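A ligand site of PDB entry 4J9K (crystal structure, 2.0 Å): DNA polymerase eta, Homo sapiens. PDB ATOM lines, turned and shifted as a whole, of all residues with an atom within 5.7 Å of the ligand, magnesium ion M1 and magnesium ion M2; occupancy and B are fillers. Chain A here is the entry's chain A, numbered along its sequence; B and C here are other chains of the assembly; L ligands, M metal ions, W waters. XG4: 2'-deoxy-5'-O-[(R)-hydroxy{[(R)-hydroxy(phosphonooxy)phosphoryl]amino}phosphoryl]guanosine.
Residues that only touch the ligand: Asp 18 (3.2 Å), Ile 51 (3.4 Å), Ala 52 (3.5 Å), Ile 117 (3.7 Å) and Leu 92 (3.9 Å).
Hydrophobic or aromatic side chains within 4 Å of the ligand: Phe 20, Phe 21, Ile 51, Ala 52, Tyr 55, Leu 92 and Ile 117.
Within 4 Å of the ligand: Asp 16, Met 17, Asp 18, Cys 19, Phe 20, Phe 21, Gln 41, Ile 51, Ala 52, Tyr 55, Arg 58, Arg 64, Leu 92, Ile 117, Asp 118, Lys 234, DT 5 of chain B, DA 6 of chain B and DT 9 of chain C.
Along chain A the residues within 4 Å of the ligand span positions 16 to 234.
The nearest printed residue that does not touch the ligand is Glu 119 (4.4 Å).
Water W6 bridges O5' of the ligand (3.1 Å) and OG of Ser 116 (3.2 Å).
Water W4 bridges O2A of the ligand and NZ of Lys 227.
Water W7 lies within hydrogen-bond range of an oxygen (O2B) of the ligand (2.7 Å), the guanidinium group (NH2) of Arg 58 (2.8 Å) and the backbone NH (N) of Val 53 (2.9 Å).
Water W8 lies within hydrogen-bond range of N3A of the ligand, O of Ile 51 and O3' of DT 9 of chain C.
Magnesium ion M1 is bound by an oxygen (O1A) of the ligand (2.0 Å), an oxygen (O1B) of the ligand (2.0 Å), an oxygen (O1G) of the ligand (2.1 Å), the side-chain carboxylate (OD1) of Asp 16 (2.1 Å), the side-chain carboxylate (OD1) of Asp 118 (2.2 Å) and the backbone carbonyl oxygen (O) of Met 17 (2.4 Å).
Magnesium ion M2 is bound by OD2 of Asp 16, 2.0 Å away.
Magnesium ion M2 is bound by the side-chain carboxylate (OE2) of Glu 119 (2.2 Å).
Magnesium ion M2 is bound by water W4.
O1A of the ligand binds magnesium ion M2, at 2.2 Å.
OD2 of Asp 118 binds magnesium ion M2, at 2.3 Å.
Water W6 is bound to magnesium ion M2 (2.5 Å).
The backbone carbonyl oxygen (O) of Asp 16 sits at hydrogen-bond distance from the side-chain amino group (NZ) of Lys 234, at 3.0 Å.
The backbone carbonyl oxygen of Met 17 lies close to the side-chain amino group of Lys 234.
N1 of DT 9 of chain C sits at hydrogen-bond distance from NH2 of Arg 64, at 3.0 Å.
N of Glu 119 lies close to OG of Ser 116 (3.2 Å).
NE2 of Gln 41 lies within hydrogen-bond range of O2 of DT 5 of chain B (3.2 Å).
The side-chain amino group (NZ) of Lys 227 lies within salt-bridge range of the side-chain carboxylate (OE1) of Glu 119, 2.8 Å away.
OG of Ser 116 lies close to N of Asp 118, at 3.1 Å.
The guanidinium group of Arg 58 sits at hydrogen-bond distance from the backbone carbonyl oxygen of Val 53 (2.8 Å).
OG of Ser 116 touches magnesium ion M2, at 3.8 Å.
Of the 25 residues printed, 4 come within 4 Å of magnesium ion M2.
NH2 of Arg 64 lies within hydrogen-bond range of O6 of the ligand, at 2.9 Å.
N of Cys 19 is in hydrogen-bond range of O2G of the ligand.
An oxygen (O2G) of the ligand is in hydrogen-bond range of the side-chain hydroxyl of Tyr 55, at 2.6 Å.
N of Phe 20 sits at hydrogen-bond distance from O2B of the ligand (3.4 Å).
NH2 of Arg 58 is in salt-bridge range of O3G of the ligand, at 3.2 Å.
The backbone NH (N) of Phe 21 sits at hydrogen-bond distance from an oxygen (O3') of the ligand, at 3.2 Å.
A nitrogen (N1) of the ligand sits at hydrogen-bond distance from N3 of DA 6 of chain B, 3.3 Å away.
The side-chain amide oxygen (OE1) of Gln 41 is in hydrogen-bond range of a nitrogen (N2) of the ligand.
O2 of DT 5 of chain B sits at hydrogen-bond distance from a nitrogen (N1) of the ligand.
The side-chain amino group (NZ) of Lys 234 lies within salt-bridge range of an oxygen (O2G) of the ligand, at 3.0 Å.
A nitrogen (N2) of the ligand is in hydrogen-bond range of O4' of DA 6 of chain B, 3.1 Å away.
O3' of DT 9 of chain C lies close to O2A of the ligand (2.7 Å).
NZ of Lys 234 touches magnesium ion M1 (3.9 Å).
Within 4 Å of magnesium ion M1: Asp 16, Met 17, Asp 118 and Lys 234.
The nearest printed residue that does not touch magnesium ion M1 is Asp 18 (4.6 Å).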
ATOM      1  N   ASP A  16     -21.452  -6.130 -35.581  1.00  0.00           N
ATOM      2  CA  ASP A  16     -20.990  -7.097 -34.587  1.00  0.00           C
ATOM      3  C   ASP A  16     -20.045  -6.477 -33.554  1.00  0.00           C
ATOM      4  O   ASP A  16     -19.047  -5.865 -33.904  1.00  0.00           O
ATOM      5  CB  ASP A  16     -20.328  -8.292 -35.287  1.00  0.00           C
ATOM      6  CG  ASP A  16     -19.861  -9.359 -34.321  1.00  0.00           C
ATOM      7  OD1 ASP A  16     -18.790  -9.189 -33.732  1.00  0.00           O
ATOM      8  OD2 ASP A  16     -20.553 -10.373 -34.139  1.00  0.00           O
ATOM      9  N   MET A  17     -20.355  -6.656 -32.276  1.00  0.00           N
ATOM     10  CA  MET A  17     -19.552  -6.078 -31.209  1.00  0.00           C
ATOM     11  C   MET A  17     -18.137  -6.652 -31.219  1.00  0.00           C
ATOM     12  O   MET A  17     -17.934  -7.829 -31.492  1.00  0.00           O
ATOM     13  CB  MET A  17     -20.214  -6.319 -29.852  1.00  0.00           C
ATOM     14  CG  MET A  17     -21.662  -5.892 -29.785  1.00  0.00           C
ATOM     15  SD  MET A  17     -21.903  -4.192 -30.339  1.00  0.00           S
ATOM     16  CE  MET A  17     -21.068  -3.274 -29.066  1.00  0.00           C
ATOM     17  N   ASP A  18     -17.153  -5.804 -30.946  1.00  0.00           N
ATOM     18  CA  ASP A  18     -15.782  -6.290 -30.825  1.00  0.00           C
ATOM     19  C   ASP A  18     -15.587  -6.993 -29.470  1.00  0.00           C
ATOM     20  O   ASP A  18     -16.048  -6.510 -28.452  1.00  0.00           O
ATOM     21  CB  ASP A  18     -14.812  -5.115 -30.988  1.00  0.00           C
ATOM     22  CG  ASP A  18     -14.943  -4.444 -32.360  1.00  0.00           C
ATOM     23  OD1 ASP A  18     -15.314  -5.131 -33.334  1.00  0.00           O
ATOM     24  OD2 ASP A  18     -14.680  -3.224 -32.464  1.00  0.00           O
ATOM     25  N   CYS A  19     -14.910  -8.142 -29.478  1.00  0.00           N
ATOM     26  CA  CYS A  19     -14.671  -8.926 -28.262  1.00  0.00           C
ATOM     27  C   CYS A  19     -15.719  -8.669 -27.179  1.00  0.00           C
ATOM     28  O   CYS A  19     -15.389  -8.265 -26.067  1.00  0.00           O
ATOM     29  CB  CYS A  19     -13.235  -8.682 -27.739  1.00  0.00           C
ATOM     30  SG  CYS A  19     -12.783  -6.953 -27.369  1.00  0.00           S
ATOM     31  N   PHE A  20     -16.975  -8.932 -27.521  1.00  0.00           N
ATOM     32  CA  PHE A  20     -18.121  -8.468 -26.739  1.00  0.00           C
ATOM     33  C   PHE A  20     -18.096  -8.719 -25.207  1.00  0.00           C
ATOM     34  O   PHE A  20     -18.216  -7.764 -24.440  1.00  0.00           O
ATOM     35  CB  PHE A  20     -19.424  -8.992 -27.342  1.00  0.00           C
ATOM     36  CG  PHE A  20     -20.665  -8.429 -26.688  1.00  0.00           C
ATOM     37  CD1 PHE A  20     -20.774  -7.067 -26.458  1.00  0.00           C
ATOM     38  CD2 PHE A  20     -21.705  -9.256 -26.327  1.00  0.00           C
ATOM     39  CE1 PHE A  20     -21.903  -6.537 -25.867  1.00  0.00           C
ATOM     40  CE2 PHE A  20     -22.846  -8.736 -25.720  1.00  0.00           C
ATOM     41  CZ  PHE A  20     -22.944  -7.370 -25.497  1.00  0.00           C
ATOM     42  N   PHE A  21     -17.976  -9.962 -24.765  1.00  0.00           N
ATOM     43  CA  PHE A  21     -18.021 -10.226 -23.320  1.00  0.00           C
ATOM     44  C   PHE A  21     -16.871  -9.508 -22.594  1.00  0.00           C
ATOM     45  O   PHE A  21     -17.043  -9.049 -21.473  1.00  0.00           O
ATOM     46  CB  PHE A  21     -18.002 -11.734 -22.993  1.00  0.00           C
ATOM     47  CG  PHE A  21     -19.296 -12.447 -23.320  1.00  0.00           C
ATOM     48  CD1 PHE A  21     -20.214 -11.892 -24.202  1.00  0.00           C
ATOM     49  CD2 PHE A  21     -19.567 -13.672 -22.753  1.00  0.00           C
ATOM     50  CE1 PHE A  21     -21.388 -12.581 -24.517  1.00  0.00           C
ATOM     51  CE2 PHE A  21     -20.740 -14.360 -23.053  1.00  0.00           C
ATOM     52  CZ  PHE A  21     -21.649 -13.808 -23.936  1.00  0.00           C
ATOM     53  N   VAL A  22     -15.703  -9.447 -23.240  1.00  0.00           N
ATOM     54  CA  VAL A  22     -14.572  -8.682 -22.700  1.00  0.00           C
ATOM     55  C   VAL A  22     -14.908  -7.190 -22.514  1.00  0.00           C
ATOM     56  O   VAL A  22     -14.654  -6.619 -21.445  1.00  0.00           O
ATOM     57  CB  VAL A  22     -13.310  -8.826 -23.579  1.00  0.00           C
ATOM     58  CG1 VAL A  22     -12.230  -7.826 -23.153  1.00  0.00           C
ATOM     59  CG2 VAL A  22     -12.763 -10.266 -23.521  1.00  0.00           C
ATOM     60  N   GLN A  41     -15.158 -19.407 -18.615  1.00  0.00           N
ATOM     61  CA  GLN A  41     -16.243 -20.034 -17.874  1.00  0.00           C
ATOM     62  C   GLN A  41     -15.636 -21.071 -16.927  1.00  0.00           C
ATOM     63  O   GLN A  41     -14.881 -21.942 -17.360  1.00  0.00           O
ATOM     64  CB  GLN A  41     -17.223 -20.727 -18.828  1.00  0.00           C
ATOM     65  CG  GLN A  41     -17.894 -19.812 -19.832  1.00  0.00           C
ATOM     66  CD  GLN A  41     -18.944 -20.521 -20.666  1.00  0.00           C
ATOM     67  OE1 GLN A  41     -20.122 -20.210 -20.602  1.00  0.00           O
ATOM     68  NE2 GLN A  41     -18.510 -21.494 -21.453  1.00  0.00           N
ATOM     69  N   ILE A  51     -13.847 -17.896 -23.731  1.00  0.00           N
ATOM     70  CA  ILE A  51     -14.878 -17.692 -24.750  1.00  0.00           C
ATOM     71  C   ILE A  51     -14.831 -16.311 -25.406  1.00  0.00           C
ATOM     72  O   ILE A  51     -15.524 -16.076 -26.400  1.00  0.00           O
ATOM     73  CB  ILE A  51     -16.310 -17.925 -24.193  1.00  0.00           C
ATOM     74  CG1 ILE A  51     -16.538 -17.047 -22.958  1.00  0.00           C
ATOM     75  CG2 ILE A  51     -16.527 -19.422 -23.894  1.00  0.00           C
ATOM     76  CD1 ILE A  51     -17.967 -17.051 -22.448  1.00  0.00           C
ATOM     77  N   ALA A  52     -14.007 -15.409 -24.877  1.00  0.00           N
ATOM     78  CA  ALA A  52     -13.815 -14.080 -25.489  1.00  0.00           C
ATOM     79  C   ALA A  52     -12.420 -13.496 -25.188  1.00  0.00           C
ATOM     80  O   ALA A  52     -11.923 -13.629 -24.075  1.00  0.00           O
ATOM     81  CB  ALA A  52     -14.914 -13.103 -25.034  1.00  0.00           C
ATOM     82  N   VAL A  53     -11.815 -12.843 -26.175  1.00  0.00           N
ATOM     83  CA  VAL A  53     -10.424 -12.401 -26.084  1.00  0.00           C
ATOM     84  C   VAL A  53     -10.209 -10.992 -26.625  1.00  0.00           C
ATOM     85  O   VAL A  53     -10.538 -10.713 -27.776  1.00  0.00           O
ATOM     86  CB  VAL A  53      -9.504 -13.367 -26.869  1.00  0.00           C
ATOM     87  CG1 VAL A  53      -8.028 -13.081 -26.580  1.00  0.00           C
ATOM     88  CG2 VAL A  53      -9.838 -14.802 -26.524  1.00  0.00           C
ATOM     89  N   TYR A  55      -8.394  -7.751 -28.234  1.00  0.00           N
ATOM     90  CA  TYR A  55      -7.448  -7.707 -29.333  1.00  0.00           C
ATOM     91  C   TYR A  55      -6.009  -7.608 -28.863  1.00  0.00           C
ATOM     92  O   TYR A  55      -5.105  -8.120 -29.525  1.00  0.00           O
ATOM     93  CB  TYR A  55      -7.836  -6.605 -30.336  1.00  0.00           C
ATOM     94  CG  TYR A  55      -9.024  -7.038 -31.159  1.00  0.00           C
ATOM     95  CD1 TYR A  55     -10.297  -7.041 -30.624  1.00  0.00           C
ATOM     96  CD2 TYR A  55      -8.856  -7.520 -32.456  1.00  0.00           C
ATOM     97  CE1 TYR A  55     -11.385  -7.461 -31.357  1.00  0.00           C
ATOM     98  CE2 TYR A  55      -9.935  -7.944 -33.203  1.00  0.00           C
ATOM     99  CZ  TYR A  55     -11.199  -7.912 -32.664  1.00  0.00           C
ATOM    100  OH  TYR A  55     -12.270  -8.350 -33.396  1.00  0.00           O
ATOM    101  N   ARG A  58      -5.164 -11.186 -28.264  1.00  0.00           N
ATOM    102  CA  ARG A  58      -5.084 -11.950 -29.519  1.00  0.00           C
ATOM    103  C   ARG A  58      -3.698 -11.801 -30.151  1.00  0.00           C
ATOM    104  O   ARG A  58      -3.214 -12.723 -30.810  1.00  0.00           O
ATOM    105  CB  ARG A  58      -6.156 -11.493 -30.518  1.00  0.00           C
ATOM    106  CG  ARG A  58      -7.580 -11.646 -30.025  1.00  0.00           C
ATOM    107  CD  ARG A  58      -8.584 -11.195 -31.071  1.00  0.00           C
ATOM    108  NE  ARG A  58      -9.929 -11.163 -30.505  1.00  0.00           N
ATOM    109  CZ  ARG A  58     -11.055 -11.113 -31.221  1.00  0.00           C
ATOM    110  NH1 ARG A  58     -11.006 -11.108 -32.540  1.00  0.00           N
ATOM    111  NH2 ARG A  58     -12.222 -11.081 -30.589  1.00  0.00           N
ATOM    112  N   ARG A  64     -10.225 -18.128 -28.511  1.00  0.00           N
ATOM    113  CA  ARG A  64     -11.392 -18.759 -27.942  1.00  0.00           C
ATOM    114  C   ARG A  64     -11.205 -20.276 -27.910  1.00  0.00           C
ATOM    115  O   ARG A  64     -10.565 -20.854 -28.784  1.00  0.00           O
ATOM    116  CB  ARG A  64     -12.624 -18.402 -28.774  1.00  0.00           C
ATOM    117  CG  ARG A  64     -13.775 -19.379 -28.670  1.00  0.00           C
ATOM    118  CD  ARG A  64     -14.915 -19.040 -29.620  1.00  0.00           C
ATOM    119  NE  ARG A  64     -16.043 -19.936 -29.446  1.00  0.00           N
ATOM    120  CZ  ARG A  64     -16.081 -21.171 -29.946  1.00  0.00           C
ATOM    121  NH1 ARG A  64     -15.075 -21.632 -30.655  1.00  0.00           N
ATOM    122  NH2 ARG A  64     -17.153 -21.925 -29.752  1.00  0.00           N
ATOM    123  N   LEU A  92     -25.184 -16.255 -17.906  1.00  0.00           N
ATOM    124  CA  LEU A  92     -24.785 -15.267 -18.897  1.00  0.00           C
ATOM    125  C   LEU A  92     -25.662 -14.010 -18.869  1.00  0.00           C
ATOM    126  O   LEU A  92     -25.648 -13.217 -19.805  1.00  0.00           O
ATOM    127  CB  LEU A  92     -24.779 -15.881 -20.301  1.00  0.00           C
ATOM    128  CG  LEU A  92     -23.847 -17.092 -20.479  1.00  0.00           C
ATOM    129  CD1 LEU A  92     -23.860 -17.610 -21.924  1.00  0.00           C
ATOM    130  CD2 LEU A  92     -22.427 -16.728 -20.042  1.00  0.00           C
ATOM    131  N   SER A 116     -27.293 -13.014 -33.135  1.00  0.00           N
ATOM    132  CA  SER A 116     -26.548 -13.608 -32.025  1.00  0.00           C
ATOM    133  C   SER A 116     -26.598 -12.668 -30.828  1.00  0.00           C
ATOM    134  O   SER A 116     -27.138 -11.568 -30.918  1.00  0.00           O
ATOM    135  CB  SER A 116     -25.095 -13.864 -32.432  1.00  0.00           C
ATOM    136  OG  SER A 116     -24.316 -12.693 -32.276  1.00  0.00           O
ATOM    137  N   ILE A 117     -26.060 -13.100 -29.695  1.00  0.00           N
ATOM    138  CA  ILE A 117     -25.982 -12.216 -28.538  1.00  0.00           C
ATOM    139  C   ILE A 117     -25.288 -10.877 -28.830  1.00  0.00           C
ATOM    140  O   ILE A 117     -25.536  -9.889 -28.120  1.00  0.00           O
ATOM    141  CB  ILE A 117     -25.266 -12.899 -27.362  1.00  0.00           C
ATOM    142  CG1 ILE A 117     -25.527 -12.125 -26.060  1.00  0.00           C
ATOM    143  CG2 ILE A 117     -23.773 -13.014 -27.647  1.00  0.00           C
ATOM    144  CD1 ILE A 117     -25.158 -12.893 -24.811  1.00  0.00           C
ATOM    145  N   ASP A 118     -24.408 -10.824 -29.839  1.00  0.00           N
ATOM    146  CA  ASP A 118     -23.661  -9.573 -30.092  1.00  0.00           C
ATOM    147  C   ASP A 118     -23.715  -8.999 -31.519  1.00  0.00           C
ATOM    148  O   ASP A 118     -22.902  -8.133 -31.882  1.00  0.00           O
ATOM    149  CB  ASP A 118     -22.193  -9.726 -29.669  1.00  0.00           C
ATOM    150  CG  ASP A 118     -21.314 -10.159 -30.805  1.00  0.00           C
ATOM    151  OD1 ASP A 118     -20.187  -9.664 -30.892  1.00  0.00           O
ATOM    152  OD2 ASP A 118     -21.748 -11.007 -31.621  1.00  0.00           O
ATOM    153  N   GLU A 119     -24.630  -9.498 -32.342  1.00  0.00           N
ATOM    154  CA  GLU A 119     -24.778  -8.983 -33.700  1.00  0.00           C
ATOM    155  C   GLU A 119     -26.209  -8.951 -34.230  1.00  0.00           C
ATOM    156  O   GLU A 119     -27.051  -9.740 -33.821  1.00  0.00           O
ATOM    157  CB  GLU A 119     -23.854  -9.726 -34.681  1.00  0.00           C
ATOM    158  CG  GLU A 119     -24.287 -11.135 -35.006  1.00  0.00           C
ATOM    159  CD  GLU A 119     -23.121 -12.019 -35.387  1.00  0.00           C
ATOM    160  OE1 GLU A 119     -22.890 -12.223 -36.589  1.00  0.00           O
ATOM    161  OE2 GLU A 119     -22.416 -12.484 -34.476  1.00  0.00           O
ATOM    162  N   LYS A 227     -21.914  -9.800 -43.601  1.00  0.00           N
ATOM    163  CA  LYS A 227     -21.220 -10.548 -42.546  1.00  0.00           C
ATOM    164  C   LYS A 227     -19.739 -10.744 -42.874  1.00  0.00           C
ATOM    165  O   LYS A 227     -18.864 -10.546 -42.018  1.00  0.00           O
ATOM    166  CB  LYS A 227     -21.892 -11.906 -42.318  1.00  0.00           C
ATOM    167  CG  LYS A 227     -21.121 -12.821 -41.377  1.00  0.00           C
ATOM    168  CD  LYS A 227     -21.007 -12.216 -39.988  1.00  0.00           C
ATOM    169  CE  LYS A 227     -20.510 -13.218 -38.951  1.00  0.00           C
ATOM    170  NZ  LYS A 227     -20.317 -12.578 -37.612  1.00  0.00           N
ATOM    171  N   LYS A 234     -12.018  -5.629 -38.590  1.00  0.00           N
ATOM    172  CA  LYS A 234     -12.119  -5.542 -37.125  1.00  0.00           C
ATOM    173  C   LYS A 234     -10.729  -5.288 -36.536  1.00  0.00           C
ATOM    174  O   LYS A 234      -9.738  -5.710 -37.112  1.00  0.00           O
ATOM    175  CB  LYS A 234     -12.714  -6.827 -36.538  1.00  0.00           C
ATOM    176  CG  LYS A 234     -14.238  -6.862 -36.538  1.00  0.00           C
ATOM    177  CD  LYS A 234     -14.759  -8.153 -35.906  1.00  0.00           C
ATOM    178  CE  LYS A 234     -16.258  -8.070 -35.583  1.00  0.00           C
ATOM    179  NZ  LYS A 234     -16.521  -7.523 -34.220  1.00  0.00           N
ATOM    180  P    DT B   4     -11.219 -31.079 -24.363  1.00  0.00           P
ATOM    181  OP1  DT B   4     -11.513 -32.292 -25.145  1.00  0.00           O
ATOM    182  OP2  DT B   4      -9.898 -30.409 -24.511  1.00  0.00           O
ATOM    183  O5'  DT B   4     -12.351 -30.001 -24.652  1.00  0.00           O
ATOM    184  C5'  DT B   4     -12.357 -28.732 -23.973  1.00  0.00           C
ATOM    185  C4'  DT B   4     -13.717 -28.074 -24.094  1.00  0.00           C
ATOM    186  O4'  DT B   4     -13.677 -27.102 -25.166  1.00  0.00           O
ATOM    187  C3'  DT B   4     -14.855 -29.031 -24.455  1.00  0.00           C
ATOM    188  O3'  DT B   4     -16.068 -28.595 -23.836  1.00  0.00           O
ATOM    189  C2'  DT B   4     -14.944 -28.916 -25.964  1.00  0.00           C
ATOM    190  C1'  DT B   4     -14.579 -27.463 -26.200  1.00  0.00           C
ATOM    191  N1   DT B   4     -13.903 -27.219 -27.487  1.00  0.00           N
ATOM    192  C2   DT B   4     -14.079 -26.000 -28.101  1.00  0.00           C
ATOM    193  O2   DT B   4     -14.764 -25.105 -27.625  1.00  0.00           O
ATOM    194  N3   DT B   4     -13.411 -25.854 -29.288  1.00  0.00           N
ATOM    195  C4   DT B   4     -12.611 -26.792 -29.926  1.00  0.00           C
ATOM    196  O4   DT B   4     -12.081 -26.515 -30.999  1.00  0.00           O
ATOM    197  C5   DT B   4     -12.471 -28.046 -29.228  1.00  0.00           C
ATOM    198  C7   DT B   4     -11.632 -29.128 -29.835  1.00  0.00           C
ATOM    199  C6   DT B   4     -13.121 -28.199 -28.070  1.00  0.00           C
ATOM    200  P    DT B   5     -16.546 -29.266 -22.466  1.00  0.00           P
ATOM    201  OP1  DT B   5     -15.362 -29.606 -21.654  1.00  0.00           O
ATOM    202  OP2  DT B   5     -17.514 -30.330 -22.823  1.00  0.00           O
ATOM    203  O5'  DT B   5     -17.348 -28.101 -21.746  1.00  0.00           O
ATOM    204  C5'  DT B   5     -16.691 -26.886 -21.351  1.00  0.00           C
ATOM    205  C4'  DT B   5     -17.711 -25.800 -21.094  1.00  0.00           C
ATOM    206  O4'  DT B   5     -17.703 -24.868 -22.204  1.00  0.00           O
ATOM    207  C3'  DT B   5     -19.163 -26.280 -20.979  1.00  0.00           C
ATOM    208  O3'  DT B   5     -19.857 -25.477 -20.019  1.00  0.00           O
ATOM    209  C2'  DT B   5     -19.709 -26.081 -22.372  1.00  0.00           C
ATOM    210  C1'  DT B   5     -18.972 -24.832 -22.823  1.00  0.00           C
ATOM    211  N1   DT B   5     -18.753 -24.735 -24.274  1.00  0.00           N
ATOM    212  C2   DT B   5     -18.984 -23.532 -24.898  1.00  0.00           C
ATOM    213  O2   DT B   5     -19.382 -22.542 -24.299  1.00  0.00           O
ATOM    214  N3   DT B   5     -18.739 -23.519 -26.245  1.00  0.00           N
ATOM    215  C4   DT B   5     -18.293 -24.574 -27.019  1.00  0.00           C
ATOM    216  O4   DT B   5     -18.107 -24.409 -28.224  1.00  0.00           O
ATOM    217  C5   DT B   5     -18.064 -25.804 -26.301  1.00  0.00           C
ATOM    218  C7   DT B   5     -17.580 -26.998 -27.068  1.00  0.00           C
ATOM    219  C6   DT B   5     -18.291 -25.818 -24.991  1.00  0.00           C
ATOM    220  P    DA B   6     -21.418 -25.624 -19.816  1.00  0.00           P
ATOM    221  OP1  DA B   6     -21.740 -25.377 -18.384  1.00  0.00           O
ATOM    222  OP2  DA B   6     -21.836 -26.910 -20.443  1.00  0.00           O
ATOM    223  O5'  DA B   6     -22.012 -24.422 -20.677  1.00  0.00           O
ATOM    224  C5'  DA B   6     -21.713 -23.060 -20.333  1.00  0.00           C
ATOM    225  C4'  DA B   6     -22.575 -22.118 -21.149  1.00  0.00           C
ATOM    226  O4'  DA B   6     -22.209 -22.196 -22.540  1.00  0.00           O
ATOM    227  C3'  DA B   6     -24.076 -22.410 -21.095  1.00  0.00           C
ATOM    228  O3'  DA B   6     -24.807 -21.183 -21.096  1.00  0.00           O
ATOM    229  C2'  DA B   6     -24.321 -23.193 -22.376  1.00  0.00           C
ATOM    230  C1'  DA B   6     -23.326 -22.556 -23.331  1.00  0.00           C
ATOM    231  N9   DA B   6     -22.866 -23.451 -24.389  1.00  0.00           N
ATOM    232  C8   DA B   6     -22.657 -24.802 -24.322  1.00  0.00           C
ATOM    233  N7   DA B   6     -22.234 -25.329 -25.448  1.00  0.00           N
ATOM    234  C5   DA B   6     -22.146 -24.247 -26.304  1.00  0.00           C
ATOM    235  C6   DA B   6     -21.754 -24.138 -27.654  1.00  0.00           C
ATOM    236  N6   DA B   6     -21.355 -25.179 -28.398  1.00  0.00           N
ATOM    237  N1   DA B   6     -21.783 -22.920 -28.221  1.00  0.00           N
ATOM    238  C2   DA B   6     -22.182 -21.879 -27.478  1.00  0.00           C
ATOM    239  N3   DA B   6     -22.575 -21.850 -26.209  1.00  0.00           N
ATOM    240  C4   DA B   6     -22.531 -23.082 -25.677  1.00  0.00           C
ATOM    241  P    DT C   9     -18.931 -18.353 -36.861  1.00  0.00           P
ATOM    242  OP1  DT C   9     -18.982 -17.004 -37.480  1.00  0.00           O
ATOM    243  OP2  DT C   9     -17.941 -19.345 -37.358  1.00  0.00           O
ATOM    244  O5'  DT C   9     -18.703 -18.166 -35.278  1.00  0.00           O
ATOM    245  C5'  DT C   9     -19.603 -17.415 -34.470  1.00  0.00           C
ATOM    246  C4'  DT C   9     -19.232 -17.544 -33.007  1.00  0.00           C
ATOM    247  O4'  DT C   9     -19.854 -18.729 -32.434  1.00  0.00           O
ATOM    248  C3'  DT C   9     -17.711 -17.659 -32.754  1.00  0.00           C
ATOM    249  O3'  DT C   9     -17.348 -17.007 -31.549  1.00  0.00           O
ATOM    250  C2'  DT C   9     -17.570 -19.143 -32.558  1.00  0.00           C
ATOM    251  C1'  DT C   9     -18.825 -19.424 -31.754  1.00  0.00           C
ATOM    252  N1   DT C   9     -19.181 -20.855 -31.656  1.00  0.00           N
ATOM    253  C2   DT C   9     -20.018 -21.239 -30.639  1.00  0.00           C
ATOM    254  O2   DT C   9     -20.506 -20.444 -29.863  1.00  0.00           O
ATOM    255  N3   DT C   9     -20.261 -22.583 -30.569  1.00  0.00           N
ATOM    256  C4   DT C   9     -19.747 -23.552 -31.419  1.00  0.00           C
ATOM    257  O4   DT C   9     -20.027 -24.728 -31.281  1.00  0.00           O
ATOM    258  C5   DT C   9     -18.859 -23.081 -32.461  1.00  0.00           C
ATOM    259  C7   DT C   9     -18.238 -24.056 -33.417  1.00  0.00           C
ATOM    260  C6   DT C   9     -18.610 -21.759 -32.522  1.00  0.00           C
HETATM  261  N1  XG4 L   1     -19.738 -20.383 -25.484  1.00  0.00           N
HETATM  262  C2  XG4 L   1     -20.312 -19.281 -24.847  1.00  0.00           C
HETATM  263  N2  XG4 L   1     -20.957 -19.586 -23.670  1.00  0.00           N
HETATM  264  N3  XG4 L   1     -20.284 -17.951 -25.235  1.00  0.00           N
HETATM  265  C4  XG4 L   1     -19.590 -17.781 -26.411  1.00  0.00           C
HETATM  266  C5  XG4 L   1     -18.980 -18.843 -27.154  1.00  0.00           C
HETATM  267  C6  XG4 L   1     -19.086 -20.142 -26.635  1.00  0.00           C
HETATM  268  O6  XG4 L   1     -18.512 -21.159 -27.293  1.00  0.00           O
HETATM  269  N7  XG4 L   1     -18.358 -18.341 -28.315  1.00  0.00           N
HETATM  270  C8  XG4 L   1     -18.592 -17.026 -28.285  1.00  0.00           C
HETATM  271  N9  XG4 L   1     -19.359 -16.604 -27.142  1.00  0.00           N
HETATM  272  PA  XG4 L   1     -18.213 -13.331 -31.394  1.00  0.00           P
HETATM  273  PB  XG4 L   1     -16.292 -11.532 -30.014  1.00  0.00           P
HETATM  274  PG  XG4 L   1     -15.064 -10.330 -32.371  1.00  0.00           P
HETATM  275  C1' XG4 L   1     -19.744 -15.231 -26.709  1.00  0.00           C
HETATM  276  O1A XG4 L   1     -18.844 -12.038 -31.990  1.00  0.00           O
HETATM  277  O1B XG4 L   1     -17.453 -10.493 -30.077  1.00  0.00           O
HETATM  278  O1G XG4 L   1     -16.493 -10.156 -32.941  1.00  0.00           O
HETATM  279  C2' XG4 L   1     -18.514 -14.441 -26.185  1.00  0.00           C
HETATM  280  O2A XG4 L   1     -18.210 -14.530 -32.262  1.00  0.00           O
HETATM  281  O2B XG4 L   1     -15.834 -11.955 -28.662  1.00  0.00           O
HETATM  282  O2G XG4 L   1     -14.547  -8.858 -32.320  1.00  0.00           O
HETATM  283  C3' XG4 L   1     -18.300 -13.415 -27.330  1.00  0.00           C
HETATM  284  O3' XG4 L   1     -17.683 -12.235 -26.943  1.00  0.00           O
HETATM  285  N3A XG4 L   1     -16.724 -12.930 -30.773  1.00  0.00           N
HETATM  286  O3B XG4 L   1     -15.134 -10.876 -30.889  1.00  0.00           O
HETATM  287  O3G XG4 L   1     -14.202 -11.296 -33.075  1.00  0.00           O
HETATM  288  C4' XG4 L   1     -19.700 -13.207 -27.918  1.00  0.00           C
HETATM  289  O4' XG4 L   1     -20.331 -14.471 -27.750  1.00  0.00           O
HETATM  290  C5' XG4 L   1     -19.877 -12.664 -29.376  1.00  0.00           C
HETATM  291  O5' XG4 L   1     -19.355 -13.638 -30.255  1.00  0.00           O
HETATM  292 MG    MG M   1     -18.280 -10.128 -31.911  1.00  0.00          MG
HETATM  293 MG    MG M   2     -20.660 -12.176 -33.227  1.00  0.00          MG
HETATM  294  O   HOH W   1     -14.270 -14.004 -32.927  1.00  0.00           O
HETATM  295  O   HOH W   2     -16.241 -14.595 -34.638  1.00  0.00           O
HETATM  296  O   HOH W   3     -21.882 -15.355 -30.121  1.00  0.00           O
HETATM  297  O   HOH W   4     -19.415 -13.189 -34.706  1.00  0.00           O
HETATM  298  O   HOH W   5     -17.164 -11.700 -35.109  1.00  0.00           O
HETATM  299  O   HOH W   6     -21.531 -14.310 -32.350  1.00  0.00           O
HETATM  300  O   HOH W   7     -13.315 -12.780 -28.672  1.00  0.00           O
HETATM  301  O   HOH W   8     -15.361 -15.273 -29.365  1.00  0.00           O
